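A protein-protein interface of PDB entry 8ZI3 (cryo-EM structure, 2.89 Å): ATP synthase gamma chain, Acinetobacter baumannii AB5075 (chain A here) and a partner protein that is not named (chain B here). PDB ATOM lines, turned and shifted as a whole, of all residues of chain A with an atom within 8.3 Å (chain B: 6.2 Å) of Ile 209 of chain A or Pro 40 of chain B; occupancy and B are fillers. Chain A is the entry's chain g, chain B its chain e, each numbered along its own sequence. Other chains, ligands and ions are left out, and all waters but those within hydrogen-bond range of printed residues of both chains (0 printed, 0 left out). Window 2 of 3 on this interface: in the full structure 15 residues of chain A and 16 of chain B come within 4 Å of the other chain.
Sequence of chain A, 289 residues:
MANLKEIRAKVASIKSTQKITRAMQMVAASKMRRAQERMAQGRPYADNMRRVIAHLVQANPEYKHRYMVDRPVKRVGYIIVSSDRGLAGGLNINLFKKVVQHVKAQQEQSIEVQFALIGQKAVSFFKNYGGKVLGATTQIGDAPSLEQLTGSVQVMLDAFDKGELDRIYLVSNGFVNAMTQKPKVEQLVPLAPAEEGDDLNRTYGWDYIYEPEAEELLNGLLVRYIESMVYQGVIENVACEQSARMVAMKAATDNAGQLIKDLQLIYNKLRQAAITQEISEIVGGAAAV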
ATOM      1  N   HIS A  55     -22.210 -25.609  23.075  1.00  0.00           N
ATOM      2  CA  HIS A  55     -22.305 -24.878  21.818  1.00  0.00           C
ATOM      3  C   HIS A  55     -23.760 -24.658  21.420  1.00  0.00           C
ATOM      4  O   HIS A  55     -24.169 -23.537  21.099  1.00  0.00           O
ATOM      5  CB  HIS A  55     -21.554 -25.658  20.736  1.00  0.00           C
ATOM      6  CG  HIS A  55     -20.836 -24.803  19.741  1.00  0.00           C
ATOM      7  ND1 HIS A  55     -19.592 -24.264  19.985  1.00  0.00           N
ATOM      8  CD2 HIS A  55     -21.163 -24.436  18.480  1.00  0.00           C
ATOM      9  CE1 HIS A  55     -19.196 -23.576  18.928  1.00  0.00           C
ATOM     10  NE2 HIS A  55     -20.130 -23.666  18.000  1.00  0.00           N
ATOM     11  N   TYR A 204     -17.799 -16.925  17.488  1.00  0.00           N
ATOM     12  CA  TYR A 204     -19.054 -17.678  17.495  1.00  0.00           C
ATOM     13  C   TYR A 204     -20.262 -16.752  17.623  1.00  0.00           C
ATOM     14  O   TYR A 204     -21.164 -16.978  18.433  1.00  0.00           O
ATOM     15  CB  TYR A 204     -19.060 -18.745  18.594  1.00  0.00           C
ATOM     16  CG  TYR A 204     -20.213 -19.714  18.474  1.00  0.00           C
ATOM     17  CD1 TYR A 204     -20.614 -20.186  17.232  1.00  0.00           C
ATOM     18  CD2 TYR A 204     -20.907 -20.145  19.596  1.00  0.00           C
ATOM     19  CE1 TYR A 204     -21.668 -21.064  17.110  1.00  0.00           C
ATOM     20  CE2 TYR A 204     -21.965 -21.027  19.483  1.00  0.00           C
ATOM     21  CZ  TYR A 204     -22.342 -21.481  18.237  1.00  0.00           C
ATOM     22  OH  TYR A 204     -23.391 -22.360  18.114  1.00  0.00           O
ATOM     23  N   TRP A 206     -22.120 -16.185  14.854  1.00  0.00           N
ATOM     24  CA  TRP A 206     -22.952 -16.551  13.715  1.00  0.00           C
ATOM     25  C   TRP A 206     -23.914 -17.692  14.016  1.00  0.00           C
ATOM     26  O   TRP A 206     -25.000 -17.745  13.424  1.00  0.00           O
ATOM     27  CB  TRP A 206     -22.067 -16.933  12.527  1.00  0.00           C
ATOM     28  CG  TRP A 206     -20.981 -17.897  12.889  1.00  0.00           C
ATOM     29  CD1 TRP A 206     -21.043 -19.257  12.836  1.00  0.00           C
ATOM     30  CD2 TRP A 206     -19.669 -17.574  13.365  1.00  0.00           C
ATOM     31  NE1 TRP A 206     -19.851 -19.803  13.247  1.00  0.00           N
ATOM     32  CE2 TRP A 206     -18.990 -18.791  13.577  1.00  0.00           C
ATOM     33  CE3 TRP A 206     -19.001 -16.374  13.632  1.00  0.00           C
ATOM     34  CZ2 TRP A 206     -17.679 -18.842  14.044  1.00  0.00           C
ATOM     35  CZ3 TRP A 206     -17.698 -16.428  14.094  1.00  0.00           C
ATOM     36  CH2 TRP A 206     -17.051 -17.654  14.295  1.00  0.00           C
ATOM     37  N   ASP A 207     -23.540 -18.601  14.910  1.00  0.00           N
ATOM     38  CA  ASP A 207     -24.356 -19.770  15.292  1.00  0.00           C
ATOM     39  C   ASP A 207     -24.582 -20.616  14.034  1.00  0.00           C
ATOM     40  O   ASP A 207     -23.661 -20.763  13.216  1.00  0.00           O
ATOM     41  CB  ASP A 207     -25.617 -19.311  15.999  1.00  0.00           C
ATOM     42  CG  ASP A 207     -25.322 -18.535  17.267  1.00  0.00           C
ATOM     43  OD1 ASP A 207     -24.161 -18.563  17.726  1.00  0.00           O
ATOM     44  OD2 ASP A 207     -26.252 -17.899  17.806  1.00  0.00           O
ATOM     45  N   TYR A 208     -25.773 -21.180  13.844  1.00  0.00           N
ATOM     46  CA  TYR A 208     -26.049 -22.067  12.725  1.00  0.00           C
ATOM     47  C   TYR A 208     -27.361 -21.672  12.063  1.00  0.00           C
ATOM     48  O   TYR A 208     -28.239 -21.066  12.683  1.00  0.00           O
ATOM     49  CB  TYR A 208     -26.112 -23.535  13.171  1.00  0.00           C
ATOM     50  CG  TYR A 208     -24.792 -24.084  13.662  1.00  0.00           C
ATOM     51  CD1 TYR A 208     -23.886 -24.658  12.781  1.00  0.00           C
ATOM     52  CD2 TYR A 208     -24.452 -24.027  15.008  1.00  0.00           C
ATOM     53  CE1 TYR A 208     -22.678 -25.161  13.224  1.00  0.00           C
ATOM     54  CE2 TYR A 208     -23.246 -24.527  15.461  1.00  0.00           C
ATOM     55  CZ  TYR A 208     -22.363 -25.093  14.565  1.00  0.00           C
ATOM     56  OH  TYR A 208     -21.162 -25.591  15.013  1.00  0.00           O
ATOM     57  N   ILE A 209     -27.485 -22.026  10.782  1.00  0.00           N
ATOM     58  CA  ILE A 209     -28.698 -21.715  10.036  1.00  0.00           C
ATOM     59  C   ILE A 209     -29.788 -22.760  10.240  1.00  0.00           C
ATOM     60  O   ILE A 209     -30.965 -22.468   9.990  1.00  0.00           O
ATOM     61  CB  ILE A 209     -28.394 -21.566   8.537  1.00  0.00           C
ATOM     62  CG1 ILE A 209     -27.399 -22.635   8.085  1.00  0.00           C
ATOM     63  CG2 ILE A 209     -27.860 -20.172   8.238  1.00  0.00           C
ATOM     64  CD1 ILE A 209     -27.058 -22.569   6.612  1.00  0.00           C
ATOM     65  N   TYR A 210     -29.429 -23.967  10.683  1.00  0.00           N
ATOM     66  CA  TYR A 210     -30.384 -25.034  10.984  1.00  0.00           C
ATOM     67  C   TYR A 210     -31.222 -25.391   9.752  1.00  0.00           C
ATOM     68  O   TYR A 210     -32.454 -25.328   9.762  1.00  0.00           O
ATOM     69  CB  TYR A 210     -31.280 -24.646  12.165  1.00  0.00           C
ATOM     70  CG  TYR A 210     -30.523 -24.263  13.414  1.00  0.00           C
ATOM     71  CD1 TYR A 210     -29.802 -25.210  14.130  1.00  0.00           C
ATOM     72  CD2 TYR A 210     -30.533 -22.957  13.881  1.00  0.00           C
ATOM     73  CE1 TYR A 210     -29.111 -24.864  15.275  1.00  0.00           C
ATOM     74  CE2 TYR A 210     -29.845 -22.601  15.024  1.00  0.00           C
ATOM     75  CZ  TYR A 210     -29.135 -23.558  15.716  1.00  0.00           C
ATOM     76  OH  TYR A 210     -28.449 -23.209  16.855  1.00  0.00           O
ATOM     77  N   GLU A 211     -30.523 -25.766   8.681  1.00  0.00           N
ATOM     78  CA  GLU A 211     -31.204 -26.102   7.431  1.00  0.00           C
ATOM     79  C   GLU A 211     -32.140 -27.299   7.555  1.00  0.00           C
ATOM     80  O   GLU A 211     -33.304 -27.185   7.132  1.00  0.00           O
ATOM     81  CB  GLU A 211     -30.164 -26.310   6.324  1.00  0.00           C
ATOM     82  CG  GLU A 211     -30.749 -26.439   4.926  1.00  0.00           C
ATOM     83  CD  GLU A 211     -31.002 -27.880   4.530  1.00  0.00           C
ATOM     84  OE1 GLU A 211     -30.230 -28.762   4.962  1.00  0.00           O
ATOM     85  OE2 GLU A 211     -31.972 -28.132   3.785  1.00  0.00           O
ATOM     86  N   PRO A 212     -31.726 -28.465   8.103  1.00  0.00           N
ATOM     87  CA  PRO A 212     -32.661 -29.601   8.165  1.00  0.00           C
ATOM     88  C   PRO A 212     -33.817 -29.362   9.122  1.00  0.00           C
ATOM     89  O   PRO A 212     -34.985 -29.512   8.747  1.00  0.00           O
ATOM     90  CB  PRO A 212     -31.776 -30.765   8.638  1.00  0.00           C
ATOM     91  CG  PRO A 212     -30.370 -30.308   8.434  1.00  0.00           C
ATOM     92  CD  PRO A 212     -30.405 -28.834   8.641  1.00  0.00           C
ATOM     93  N   GLU A 213     -33.504 -28.987  10.361  1.00  0.00           N
ATOM     94  CA  GLU A 213     -34.514 -28.693  11.365  1.00  0.00           C
ATOM     95  C   GLU A 213     -34.058 -27.503  12.193  1.00  0.00           C
ATOM     96  O   GLU A 213     -32.865 -27.329  12.451  1.00  0.00           O
ATOM     97  CB  GLU A 213     -34.779 -29.899  12.278  1.00  0.00           C
ATOM     98  CG  GLU A 213     -35.645 -30.979  11.651  1.00  0.00           C
ATOM     99  CD  GLU A 213     -34.827 -32.096  11.036  1.00  0.00           C
ATOM    100  OE1 GLU A 213     -33.582 -32.013  11.074  1.00  0.00           O
ATOM    101  OE2 GLU A 213     -35.430 -33.056  10.512  1.00  0.00           O
ATOM    102  N   ALA A 214     -35.025 -26.687  12.616  1.00  0.00           N
ATOM    103  CA  ALA A 214     -34.699 -25.491  13.387  1.00  0.00           C
ATOM    104  C   ALA A 214     -34.223 -25.854  14.788  1.00  0.00           C
ATOM    105  O   ALA A 214     -33.085 -25.554  15.170  1.00  0.00           O
ATOM    106  CB  ALA A 214     -35.911 -24.561  13.448  1.00  0.00           C
ATOM    107  N   GLU A 215     -35.086 -26.505  15.575  1.00  0.00           N
ATOM    108  CA  GLU A 215     -34.736 -26.911  16.931  1.00  0.00           C
ATOM    109  C   GLU A 215     -35.304 -28.285  17.269  1.00  0.00           C
ATOM    110  O   GLU A 215     -35.631 -28.556  18.430  1.00  0.00           O
ATOM    111  CB  GLU A 215     -35.217 -25.882  17.956  1.00  0.00           C
ATOM    112  CG  GLU A 215     -34.301 -24.678  18.112  1.00  0.00           C
ATOM    113  CD  GLU A 215     -34.636 -23.557  17.148  1.00  0.00           C
ATOM    114  OE1 GLU A 215     -35.770 -23.540  16.624  1.00  0.00           O
ATOM    115  OE2 GLU A 215     -33.766 -22.692  16.915  1.00  0.00           O
ATOM    116  N   HIS B  38     -17.286 -21.477   5.228  1.00  0.00           N
ATOM    117  CA  HIS B  38     -18.434 -20.608   5.435  1.00  0.00           C
ATOM    118  C   HIS B  38     -19.679 -21.475   5.562  1.00  0.00           C
ATOM    119  O   HIS B  38     -19.652 -22.680   5.299  1.00  0.00           O
ATOM    120  CB  HIS B  38     -18.580 -19.592   4.298  1.00  0.00           C
ATOM    121  CG  HIS B  38     -18.860 -20.214   2.964  1.00  0.00           C
ATOM    122  ND1 HIS B  38     -20.130 -20.557   2.554  1.00  0.00           N
ATOM    123  CD2 HIS B  38     -18.032 -20.552   1.948  1.00  0.00           C
ATOM    124  CE1 HIS B  38     -20.073 -21.081   1.343  1.00  0.00           C
ATOM    125  NE2 HIS B  38     -18.811 -21.090   0.952  1.00  0.00           N
ATOM    126  N   ALA B  39     -20.775 -20.838   5.980  1.00  0.00           N
ATOM    127  CA  ALA B  39     -22.077 -21.471   6.155  1.00  0.00           C
ATOM    128  C   ALA B  39     -22.006 -22.639   7.133  1.00  0.00           C
ATOM    129  O   ALA B  39     -22.120 -23.800   6.717  1.00  0.00           O
ATOM    130  CB  ALA B  39     -22.635 -21.941   4.809  1.00  0.00           C
ATOM    131  N   PRO B  40     -21.803 -22.382   8.426  1.00  0.00           N
ATOM    132  CA  PRO B  40     -21.860 -23.470   9.408  1.00  0.00           C
ATOM    133  C   PRO B  40     -23.239 -24.110   9.428  1.00  0.00           C
ATOM    134  O   PRO B  40     -24.261 -23.438   9.275  1.00  0.00           O
ATOM    135  CB  PRO B  40     -21.548 -22.771  10.737  1.00  0.00           C
ATOM    136  CG  PRO B  40     -20.903 -21.478  10.354  1.00  0.00           C
ATOM    137  CD  PRO B  40     -21.531 -21.083   9.061  1.00  0.00           C
ATOM    138  N   LEU B  41     -23.261 -25.426   9.623  1.00  0.00           N
ATOM    139  CA  LEU B  41     -24.511 -26.162   9.508  1.00  0.00           C
ATOM    140  C   LEU B  41     -24.349 -27.514  10.192  1.00  0.00           C
ATOM    141  O   LEU B  41     -23.235 -28.011  10.370  1.00  0.00           O
ATOM    142  CB  LEU B  41     -24.909 -26.307   8.030  1.00  0.00           C
ATOM    143  CG  LEU B  41     -26.193 -26.993   7.555  1.00  0.00           C
ATOM    144  CD1 LEU B  41     -25.985 -28.479   7.341  1.00  0.00           C
ATOM    145  CD2 LEU B  41     -27.355 -26.721   8.501  1.00  0.00           C
ATOM    146  N   VAL B  42     -25.480 -28.094  10.590  1.00  0.00           N
ATOM    147  CA  VAL B  42     -25.530 -29.408  11.220  1.00  0.00           C
ATOM    148  C   VAL B  42     -26.597 -30.238  10.521  1.00  0.00           C
ATOM    149  O   VAL B  42     -27.660 -29.720  10.159  1.00  0.00           O
ATOM    150  CB  VAL B  42     -25.818 -29.307  12.733  1.00  0.00           C
ATOM    151  CG1 VAL B  42     -24.564 -28.890  13.483  1.00  0.00           C
ATOM    152  CG2 VAL B  42     -26.949 -28.325  12.994  1.00  0.00           C
ATOM    153  N   VAL B  71     -20.687 -29.362  10.633  1.00  0.00           N
ATOM    154  CA  VAL B  71     -19.714 -28.751   9.737  1.00  0.00           C
ATOM    155  C   VAL B  71     -19.653 -27.259  10.035  1.00  0.00           C
ATOM    156  O   VAL B  71     -20.684 -26.612  10.248  1.00  0.00           O
ATOM    157  CB  VAL B  71     -20.045 -29.018   8.249  1.00  0.00           C
ATOM    158  CG1 VAL B  71     -21.379 -28.400   7.854  1.00  0.00           C
ATOM    159  CG2 VAL B  71     -18.927 -28.509   7.352  1.00  0.00           C
ATOM    160  N   GLN B  72     -18.436 -26.724  10.081  1.00  0.00           N
ATOM    161  CA  GLN B  72     -18.204 -25.330  10.431  1.00  0.00           C
ATOM    162  C   GLN B  72     -16.849 -24.931   9.870  1.00  0.00           C
ATOM    163  O   GLN B  72     -15.983 -25.796   9.695  1.00  0.00           O
ATOM    164  CB  GLN B  72     -18.242 -25.134  11.956  1.00  0.00           C
ATOM    165  CG  GLN B  72     -18.489 -23.708  12.423  1.00  0.00           C
ATOM    166  CD  GLN B  72     -17.206 -22.967  12.740  1.00  0.00           C
ATOM    167  OE1 GLN B  72     -16.246 -23.552  13.242  1.00  0.00           O
ATOM    168  NE2 GLN B  72     -17.182 -21.672  12.445  1.00  0.00           N
ATOM    169  N   PRO B  73     -16.645 -23.648   9.540  1.00  0.00           N
ATOM    170  CA  PRO B  73     -15.310 -23.195   9.126  1.00  0.00           C
ATOM    171  C   PRO B  73     -14.211 -23.629  10.084  1.00  0.00           C
ATOM    172  O   PRO B  73     -14.209 -23.243  11.257  1.00  0.00           O
ATOM    173  CB  PRO B  73     -15.455 -21.670   9.098  1.00  0.00           C
ATOM    174  CG  PRO B  73     -16.899 -21.436   8.795  1.00  0.00           C
ATOM    175  CD  PRO B  73     -17.684 -22.645   9.243  1.00  0.00           C
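NE2 of Gln 72 of chain B lies close to NE1 of Trp 206 of chain A.
N of Val 71 of chain B lies within hydrogen-bond range of O of Leu 41 of chain B, at 2.9 Å.
Among the printed residues, pairs that only touch across the chains: Pro 212 of chain A with Val 42 of chain B, Tyr 208 of chain A with Leu 41 of chain B, Glu 211 of chain A with Leu 41 of chain B, Trp 206 of chain A with Pro 40 of chain B, Ile 209 of chain A with Pro 40 of chain B, Tyr 208 of chain A with Pro 40 of chain B, Pro 212 of chain A with Leu 41 of chain B, Asp 207 of chain A with Pro 40 of chain B and Tyr 208 of chain A with Val 71 of chain B.
Of the printed residues of chain B, Ile 209 of chain A touches Pro 40 (3.5 Å). Of chain A, only Trp 206 (3.3 Å), Asp 207 (3.8 Å), Tyr 208 (3.5 Å) and Ile 209 (3.5 Å) come within 4 Å of Pro 40 of chain B. Of the printed residues of chain B, Trp 206 of chain A touches Pro 40 (3.3 Å) and Gln 72 (3.3 Å). Printed residues of chain A within 4 Å of Val 71 of chain B: Tyr 208. Printed residues of chain B within 4 Å of Asp 207 of chain A: Pro 40. Printed residues of chain B within 4 Å of Tyr 208 of chain A: Pro 40 (3.5 Å), Leu 41 (3.3 Å) and Val 71 (3.9 Å). Ala 214 of chain A touches none of the printed residues of chain B. The nearest residue of chain A that does not touch Pro 40 of chain B is Tyr 210 of chain A (5.4 Å).
Of the 8 printed residues of chain B, 5 touch a printed residue of chain A. Printed residues of chain B that touch a printed residue of chain A: Pro 40, Leu 41, Val 42, Val 71 and Gln 72. Hydrophobic or aromatic side chains of chain B within 4 Å of the printed part of chain A: Pro 40 and Leu 41. Among the printed residues, 10 pairs touch across the chains.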
